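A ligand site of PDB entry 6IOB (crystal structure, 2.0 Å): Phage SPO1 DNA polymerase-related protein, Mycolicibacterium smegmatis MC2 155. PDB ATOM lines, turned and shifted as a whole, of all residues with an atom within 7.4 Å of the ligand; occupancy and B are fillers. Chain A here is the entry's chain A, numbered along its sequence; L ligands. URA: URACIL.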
ATOM      1  N   VAL A  40      35.390  24.625  26.096  1.00  0.00           N
ATOM      2  CA  VAL A  40      34.945  23.307  25.662  1.00  0.00           C
ATOM      3  C   VAL A  40      35.730  23.039  24.382  1.00  0.00           C
ATOM      4  O   VAL A  40      35.373  23.482  23.286  1.00  0.00           O
ATOM      5  CB  VAL A  40      33.435  23.278  25.413  1.00  0.00           C
ATOM      6  CG1 VAL A  40      32.986  21.908  24.862  1.00  0.00           C
ATOM      7  CG2 VAL A  40      32.646  23.651  26.663  1.00  0.00           C
ATOM      8  N   ILE A  53      32.403  19.610  13.108  1.00  0.00           N
ATOM      9  CA  ILE A  53      32.414  20.953  13.682  1.00  0.00           C
ATOM     10  C   ILE A  53      30.983  21.475  13.868  1.00  0.00           C
ATOM     11  O   ILE A  53      30.218  21.593  12.890  1.00  0.00           O
ATOM     12  CB  ILE A  53      33.192  21.937  12.810  1.00  0.00           C
ATOM     13  CG1 ILE A  53      34.590  21.386  12.530  1.00  0.00           C
ATOM     14  CG2 ILE A  53      33.366  23.234  13.587  1.00  0.00           C
ATOM     15  CD1 ILE A  53      35.392  22.208  11.571  1.00  0.00           C
ATOM     16  N   GLY A  54      30.608  21.723  15.137  1.00  0.00           N
ATOM     17  CA  GLY A  54      29.356  22.367  15.497  1.00  0.00           C
ATOM     18  C   GLY A  54      29.483  23.870  15.674  1.00  0.00           C
ATOM     19  O   GLY A  54      30.438  24.496  15.205  1.00  0.00           O
ATOM     20  N   GLU A  55      28.487  24.466  16.349  1.00  0.00           N
ATOM     21  CA  GLU A  55      28.417  25.919  16.535  1.00  0.00           C
ATOM     22  C   GLU A  55      29.117  26.397  17.814  1.00  0.00           C
ATOM     23  O   GLU A  55      30.099  27.136  17.757  1.00  0.00           O
ATOM     24  CB  GLU A  55      26.960  26.405  16.482  1.00  0.00           C
ATOM     25  CG  GLU A  55      26.856  27.911  16.693  1.00  0.00           C
ATOM     26  CD  GLU A  55      25.445  28.443  16.566  1.00  0.00           C
ATOM     27  OE1 GLU A  55      24.892  28.255  15.475  1.00  0.00           O
ATOM     28  OE2 GLU A  55      24.832  28.924  17.556  1.00  0.00           O
ATOM     29  N   GLN A  56      28.647  25.940  18.969  1.00  0.00           N
ATOM     30  CA  GLN A  56      29.151  26.409  20.255  1.00  0.00           C
ATOM     31  C   GLN A  56      28.633  25.450  21.310  1.00  0.00           C
ATOM     32  O   GLN A  56      27.739  24.654  21.047  1.00  0.00           O
ATOM     33  CB  GLN A  56      28.705  27.849  20.568  1.00  0.00           C
ATOM     34  CG  GLN A  56      27.231  28.032  20.913  1.00  0.00           C
ATOM     35  CD  GLN A  56      27.062  29.039  22.030  1.00  0.00           C
ATOM     36  OE1 GLN A  56      27.958  29.206  22.845  1.00  0.00           O
ATOM     37  NE2 GLN A  56      25.881  29.648  22.121  1.00  0.00           N
ATOM     38  N   PRO A  57      29.184  25.485  22.521  1.00  0.00           N
ATOM     39  CA  PRO A  57      28.637  24.661  23.610  1.00  0.00           C
ATOM     40  C   PRO A  57      27.236  25.069  24.012  1.00  0.00           C
ATOM     41  O   PRO A  57      26.778  26.175  23.774  1.00  0.00           O
ATOM     42  CB  PRO A  57      29.625  24.849  24.756  1.00  0.00           C
ATOM     43  CG  PRO A  57      30.729  25.712  24.244  1.00  0.00           C
ATOM     44  CD  PRO A  57      30.283  26.345  22.990  1.00  0.00           C
ATOM     45  N   GLY A  58      26.506  24.092  24.559  1.00  0.00           N
ATOM     46  CA  GLY A  58      25.301  24.397  25.289  1.00  0.00           C
ATOM     47  C   GLY A  58      25.576  24.313  26.780  1.00  0.00           C
ATOM     48  O   GLY A  58      26.723  24.232  27.238  1.00  0.00           O
ATOM     49  N   ASP A  59      24.489  24.321  27.547  1.00  0.00           N
ATOM     50  CA  ASP A  59      24.572  24.344  29.011  1.00  0.00           C
ATOM     51  C   ASP A  59      25.397  23.154  29.516  1.00  0.00           C
ATOM     52  O   ASP A  59      26.401  23.321  30.220  1.00  0.00           O
ATOM     53  CB  ASP A  59      23.173  24.409  29.596  1.00  0.00           C
ATOM     54  CG  ASP A  59      23.157  24.359  31.102  1.00  0.00           C
ATOM     55  OD1 ASP A  59      22.210  23.758  31.655  1.00  0.00           O
ATOM     56  OD2 ASP A  59      24.044  24.978  31.748  1.00  0.00           O
ATOM     57  N   GLU A  61      27.273  21.056  27.844  1.00  0.00           N
ATOM     58  CA  GLU A  61      28.628  21.060  27.322  1.00  0.00           C
ATOM     59  C   GLU A  61      29.540  21.909  28.208  1.00  0.00           C
ATOM     60  O   GLU A  61      30.683  21.525  28.492  1.00  0.00           O
ATOM     61  CB  GLU A  61      28.646  21.574  25.892  1.00  0.00           C
ATOM     62  CG  GLU A  61      28.111  20.597  24.857  1.00  0.00           C
ATOM     63  CD  GLU A  61      26.610  20.483  24.897  1.00  0.00           C
ATOM     64  OE1 GLU A  61      25.968  21.394  25.455  1.00  0.00           O
ATOM     65  OE2 GLU A  61      26.076  19.519  24.318  1.00  0.00           O
ATOM     66  N   LEU A  66      33.064  19.125  27.213  1.00  0.00           N
ATOM     67  CA  LEU A  66      33.123  18.299  26.013  1.00  0.00           C
ATOM     68  C   LEU A  66      31.973  18.624  25.079  1.00  0.00           C
ATOM     69  O   LEU A  66      30.908  19.040  25.544  1.00  0.00           O
ATOM     70  CB  LEU A  66      33.150  16.783  26.215  1.00  0.00           C
ATOM     71  CG  LEU A  66      34.361  16.166  26.872  1.00  0.00           C
ATOM     72  CD1 LEU A  66      34.011  14.741  27.311  1.00  0.00           C
ATOM     73  CD2 LEU A  66      35.505  16.190  25.864  1.00  0.00           C
ATOM     74  N   PRO A  67      32.157  18.474  23.783  1.00  0.00           N
ATOM     75  CA  PRO A  67      31.079  18.822  22.873  1.00  0.00           C
ATOM     76  C   PRO A  67      30.057  17.691  22.751  1.00  0.00           C
ATOM     77  O   PRO A  67      30.346  16.505  22.941  1.00  0.00           O
ATOM     78  CB  PRO A  67      31.819  19.030  21.537  1.00  0.00           C
ATOM     79  CG  PRO A  67      33.009  18.077  21.648  1.00  0.00           C
ATOM     80  CD  PRO A  67      33.415  18.115  23.095  1.00  0.00           C
ATOM     81  N   PHE A  68      28.842  18.118  22.400  1.00  0.00           N
ATOM     82  CA  PHE A  68      27.742  17.217  22.039  1.00  0.00           C
ATOM     83  C   PHE A  68      27.471  16.151  23.119  1.00  0.00           C
ATOM     84  O   PHE A  68      27.429  14.960  22.841  1.00  0.00           O
ATOM     85  CB  PHE A  68      27.983  16.584  20.664  1.00  0.00           C
ATOM     86  CG  PHE A  68      27.684  17.523  19.533  1.00  0.00           C
ATOM     87  CD1 PHE A  68      26.378  17.867  19.209  1.00  0.00           C
ATOM     88  CD2 PHE A  68      28.720  18.065  18.789  1.00  0.00           C
ATOM     89  CE1 PHE A  68      26.123  18.735  18.167  1.00  0.00           C
ATOM     90  CE2 PHE A  68      28.465  18.933  17.748  1.00  0.00           C
ATOM     91  CZ  PHE A  68      27.174  19.270  17.428  1.00  0.00           C
ATOM     92  N   VAL A  69      27.250  16.617  24.344  1.00  0.00           N
ATOM     93  CA  VAL A  69      26.869  15.713  25.439  1.00  0.00           C
ATOM     94  C   VAL A  69      25.403  15.823  25.813  1.00  0.00           C
ATOM     95  O   VAL A  69      24.925  15.045  26.644  1.00  0.00           O
ATOM     96  CB  VAL A  69      27.746  15.941  26.686  1.00  0.00           C
ATOM     97  CG1 VAL A  69      29.177  15.602  26.391  1.00  0.00           C
ATOM     98  CG2 VAL A  69      27.651  17.376  27.142  1.00  0.00           C
ATOM     99  N   GLY A  70      24.673  16.789  25.278  1.00  0.00           N
ATOM    100  CA  GLY A  70      23.255  16.897  25.555  1.00  0.00           C
ATOM    101  C   GLY A  70      22.341  16.253  24.541  1.00  0.00           C
ATOM    102  O   GLY A  70      22.720  15.315  23.823  1.00  0.00           O
ATOM    103  N   ALA A  72      21.178  17.253  21.669  1.00  0.00           N
ATOM    104  CA  ALA A  72      21.718  17.309  20.331  1.00  0.00           C
ATOM    105  C   ALA A  72      22.774  16.246  20.118  1.00  0.00           C
ATOM    106  O   ALA A  72      22.839  15.634  19.046  1.00  0.00           O
ATOM    107  CB  ALA A  72      22.311  18.704  20.082  1.00  0.00           C
ATOM    108  N   GLY A  73      23.589  15.969  21.151  1.00  0.00           N
ATOM    109  CA  GLY A  73      24.567  14.904  21.015  1.00  0.00           C
ATOM    110  C   GLY A  73      23.990  13.500  20.931  1.00  0.00           C
ATOM    111  O   GLY A  73      24.493  12.671  20.172  1.00  0.00           O
ATOM    112  N   ARG A  87      31.770   7.032  16.803  1.00  0.00           N
ATOM    113  CA  ARG A  87      32.018   8.376  17.310  1.00  0.00           C
ATOM    114  C   ARG A  87      33.433   8.538  17.827  1.00  0.00           C
ATOM    115  O   ARG A  87      34.051   9.603  17.665  1.00  0.00           O
ATOM    116  CB  ARG A  87      31.015   8.730  18.411  1.00  0.00           C
ATOM    117  CG  ARG A  87      31.225  10.135  18.966  1.00  0.00           C
ATOM    118  CD  ARG A  87      30.002  10.649  19.715  1.00  0.00           C
ATOM    119  NE  ARG A  87      30.253  11.883  20.459  1.00  0.00           N
ATOM    120  CZ  ARG A  87      29.307  12.588  21.048  1.00  0.00           C
ATOM    121  NH1 ARG A  87      28.042  12.182  20.987  1.00  0.00           N
ATOM    122  NH2 ARG A  87      29.600  13.702  21.719  1.00  0.00           N
ATOM    123  N   VAL A  92      35.501  15.614  17.171  1.00  0.00           N
ATOM    124  CA  VAL A  92      34.302  16.434  17.281  1.00  0.00           C
ATOM    125  C   VAL A  92      34.650  17.705  18.037  1.00  0.00           C
ATOM    126  O   VAL A  92      35.174  17.650  19.162  1.00  0.00           O
ATOM    127  CB  VAL A  92      33.178  15.653  17.974  1.00  0.00           C
ATOM    128  CG1 VAL A  92      31.963  16.491  18.188  1.00  0.00           C
ATOM    129  CG2 VAL A  92      32.775  14.480  17.143  1.00  0.00           C
ATOM    130  N   THR A  93      34.352  18.854  17.439  1.00  0.00           N
ATOM    131  CA  THR A  93      34.601  20.134  18.097  1.00  0.00           C
ATOM    132  C   THR A  93      33.538  21.140  17.660  1.00  0.00           C
ATOM    133  O   THR A  93      32.569  20.804  16.974  1.00  0.00           O
ATOM    134  CB  THR A  93      36.026  20.604  17.785  1.00  0.00           C
ATOM    135  OG1 THR A  93      36.392  21.662  18.675  1.00  0.00           O
ATOM    136  CG2 THR A  93      36.124  21.084  16.343  1.00  0.00           C
ATOM    137  N   ASN A  94      33.755  22.396  18.049  1.00  0.00           N
ATOM    138  CA  ASN A  94      32.827  23.477  17.761  1.00  0.00           C
ATOM    139  C   ASN A  94      33.593  24.683  17.243  1.00  0.00           C
ATOM    140  O   ASN A  94      34.794  24.844  17.515  1.00  0.00           O
ATOM    141  CB  ASN A  94      32.032  23.910  19.003  1.00  0.00           C
ATOM    142  CG  ASN A  94      30.984  22.903  19.413  1.00  0.00           C
ATOM    143  OD1 ASN A  94      30.130  22.507  18.624  1.00  0.00           O
ATOM    144  ND2 ASN A  94      31.050  22.471  20.666  1.00  0.00           N
ATOM    145  N   ALA A  95      32.910  25.507  16.449  1.00  0.00           N
ATOM    146  CA  ALA A  95      33.537  26.716  15.946  1.00  0.00           C
ATOM    147  C   ALA A  95      33.946  27.650  17.078  1.00  0.00           C
ATOM    148  O   ALA A  95      34.947  28.356  16.969  1.00  0.00           O
ATOM    149  CB  ALA A  95      32.617  27.438  14.959  1.00  0.00           C
ATOM    150  N   VAL A  96      33.114  27.726  18.117  1.00  0.00           N
ATOM    151  CA  VAL A  96      33.341  28.603  19.261  1.00  0.00           C
ATOM    152  C   VAL A  96      33.450  27.730  20.506  1.00  0.00           C
ATOM    153  O   VAL A  96      32.635  26.827  20.709  1.00  0.00           O
ATOM    154  CB  VAL A  96      32.179  29.613  19.377  1.00  0.00           C
ATOM    155  CG1 VAL A  96      32.138  30.287  20.722  1.00  0.00           C
ATOM    156  CG2 VAL A  96      32.266  30.638  18.234  1.00  0.00           C
ATOM    157  N   LEU A 142      28.478  21.007  10.619  1.00  0.00           N
ATOM    158  CA  LEU A 142      27.105  20.871  11.104  1.00  0.00           C
ATOM    159  C   LEU A 142      26.496  22.247  11.312  1.00  0.00           C
ATOM    160  O   LEU A 142      26.705  22.874  12.355  1.00  0.00           O
ATOM    161  CB  LEU A 142      27.087  20.071  12.403  1.00  0.00           C
ATOM    162  CG  LEU A 142      27.765  18.706  12.340  1.00  0.00           C
ATOM    163  CD1 LEU A 142      27.972  18.177  13.739  1.00  0.00           C
ATOM    164  CD2 LEU A 142      26.913  17.730  11.526  1.00  0.00           C
ATOM    165  N   ALA A 146      29.231  26.835  11.757  1.00  0.00           N
ATOM    166  CA  ALA A 146      30.474  26.123  11.444  1.00  0.00           C
ATOM    167  C   ALA A 146      30.849  26.262   9.970  1.00  0.00           C
ATOM    168  O   ALA A 146      32.023  26.532   9.613  1.00  0.00           O
ATOM    169  CB  ALA A 146      30.330  24.652  11.817  1.00  0.00           C
ATOM    170  N   HIS A 181      22.582  21.082  11.322  1.00  0.00           N
ATOM    171  CA  HIS A 181      22.978  20.927  12.718  1.00  0.00           C
ATOM    172  C   HIS A 181      21.997  20.009  13.438  1.00  0.00           C
ATOM    173  O   HIS A 181      20.781  20.134  13.260  1.00  0.00           O
ATOM    174  CB  HIS A 181      23.073  22.308  13.409  1.00  0.00           C
ATOM    175  CG  HIS A 181      23.708  22.274  14.780  1.00  0.00           C
ATOM    176  ND1 HIS A 181      23.119  21.658  15.855  1.00  0.00           N
ATOM    177  CD2 HIS A 181      24.909  22.728  15.215  1.00  0.00           C
ATOM    178  CE1 HIS A 181      23.900  21.761  16.914  1.00  0.00           C
ATOM    179  NE2 HIS A 181      25.000  22.396  16.556  1.00  0.00           N
ATOM    180  N   PRO A 182      22.493  19.029  14.202  1.00  0.00           N
ATOM    181  CA  PRO A 182      21.597  18.115  14.940  1.00  0.00           C
ATOM    182  C   PRO A 182      20.530  18.786  15.776  1.00  0.00           C
ATOM    183  O   PRO A 182      19.430  18.233  15.894  1.00  0.00           O
ATOM    184  CB  PRO A 182      22.568  17.310  15.818  1.00  0.00           C
ATOM    185  CG  PRO A 182      23.867  17.351  15.081  1.00  0.00           C
ATOM    186  CD  PRO A 182      23.921  18.661  14.355  1.00  0.00           C
ATOM    187  N   SER A 183      20.828  19.936  16.401  1.00  0.00           N
ATOM    188  CA  SER A 183      19.818  20.643  17.180  1.00  0.00           C
ATOM    189  C   SER A 183      18.613  21.012  16.324  1.00  0.00           C
ATOM    190  O   SER A 183      17.472  21.043  16.821  1.00  0.00           O
ATOM    191  CB  SER A 183      20.427  21.916  17.794  1.00  0.00           C
ATOM    192  OG  SER A 183      21.313  21.611  18.850  1.00  0.00           O
HETATM  193  N1  URA L   1      25.417  22.683  19.890  1.00  0.00           N
HETATM  194  C2  URA L   1      26.719  22.671  19.184  1.00  0.00           C
HETATM  195  O2  URA L   1      26.874  23.249  18.163  1.00  0.00           O
HETATM  196  N3  URA L   1      27.876  21.938  19.755  1.00  0.00           N
HETATM  197  C4  URA L   1      27.723  21.218  21.014  1.00  0.00           C
HETATM  198  O4  URA L   1      28.643  20.623  21.469  1.00  0.00           O
HETATM  199  C5  URA L   1      26.403  21.227  21.705  1.00  0.00           C
HETATM  200  C6  URA L   1      25.298  21.949  21.145  1.00  0.00           C
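A ring nitrogen (NE2) of His 181 sits at hydrogen-bond distance from an oxygen (O2) of the ligand (2.6 Å). An oxygen (O4) of the ligand is in hydrogen-bond range of the backbone NH (N) of Phe 68 (2.7 Å). The backbone carbonyl oxygen of Gln 56 sits close to a nitrogen (N3) of the ligand, 3.0 Å away. The backbone NH of Glu 55 lies within hydrogen-bond range of an oxygen (O2) of the ligand. O2 of the ligand sits at hydrogen-bond distance from N of Gln 56, at 3.3 Å. OD1 of Asn 94 sits at hydrogen-bond distance from N3 of the ligand (2.6 Å).
O of Gly 54 sits at hydrogen-bond distance from N of Ala 95, at 2.9 Å. The backbone NH (N) of Val 69 lies within hydrogen-bond range of the side-chain carboxylate (OE2) of Glu 61 (3.1 Å). N of Val 96 lies within hydrogen-bond range of O of Glu 55 (3.1 Å). A ring nitrogen (ND1) of His 181 sits at hydrogen-bond distance from the backbone NH (N) of Ser 183, at 2.9 Å. NH2 of Arg 87 is in hydrogen-bond range of O of Pro 67, at 3.1 Å. OE1 of Glu 61 is in hydrogen-bond range of N of Gly 58, at 2.9 Å. The backbone NH of Gly 70 sits at hydrogen-bond distance from the side-chain carboxylate of Glu 61 (3.2 Å). The side-chain amide oxygen of Asn 94 sits at hydrogen-bond distance from the backbone NH of Glu 55 (3.4 Å).
Gly 54 touches the ligand. Glu 61 touches the ligand. CA of Pro 67 touches O4 of the ligand, 3.3 Å away. Within 4 Å of the ligand: Gly 54, Glu 55, Gln 56, Glu 61, Pro 67, Phe 68, Asn 94 and His 181. The nearest printed residue that does not touch the ligand is Gly 58 (4.05 Å).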
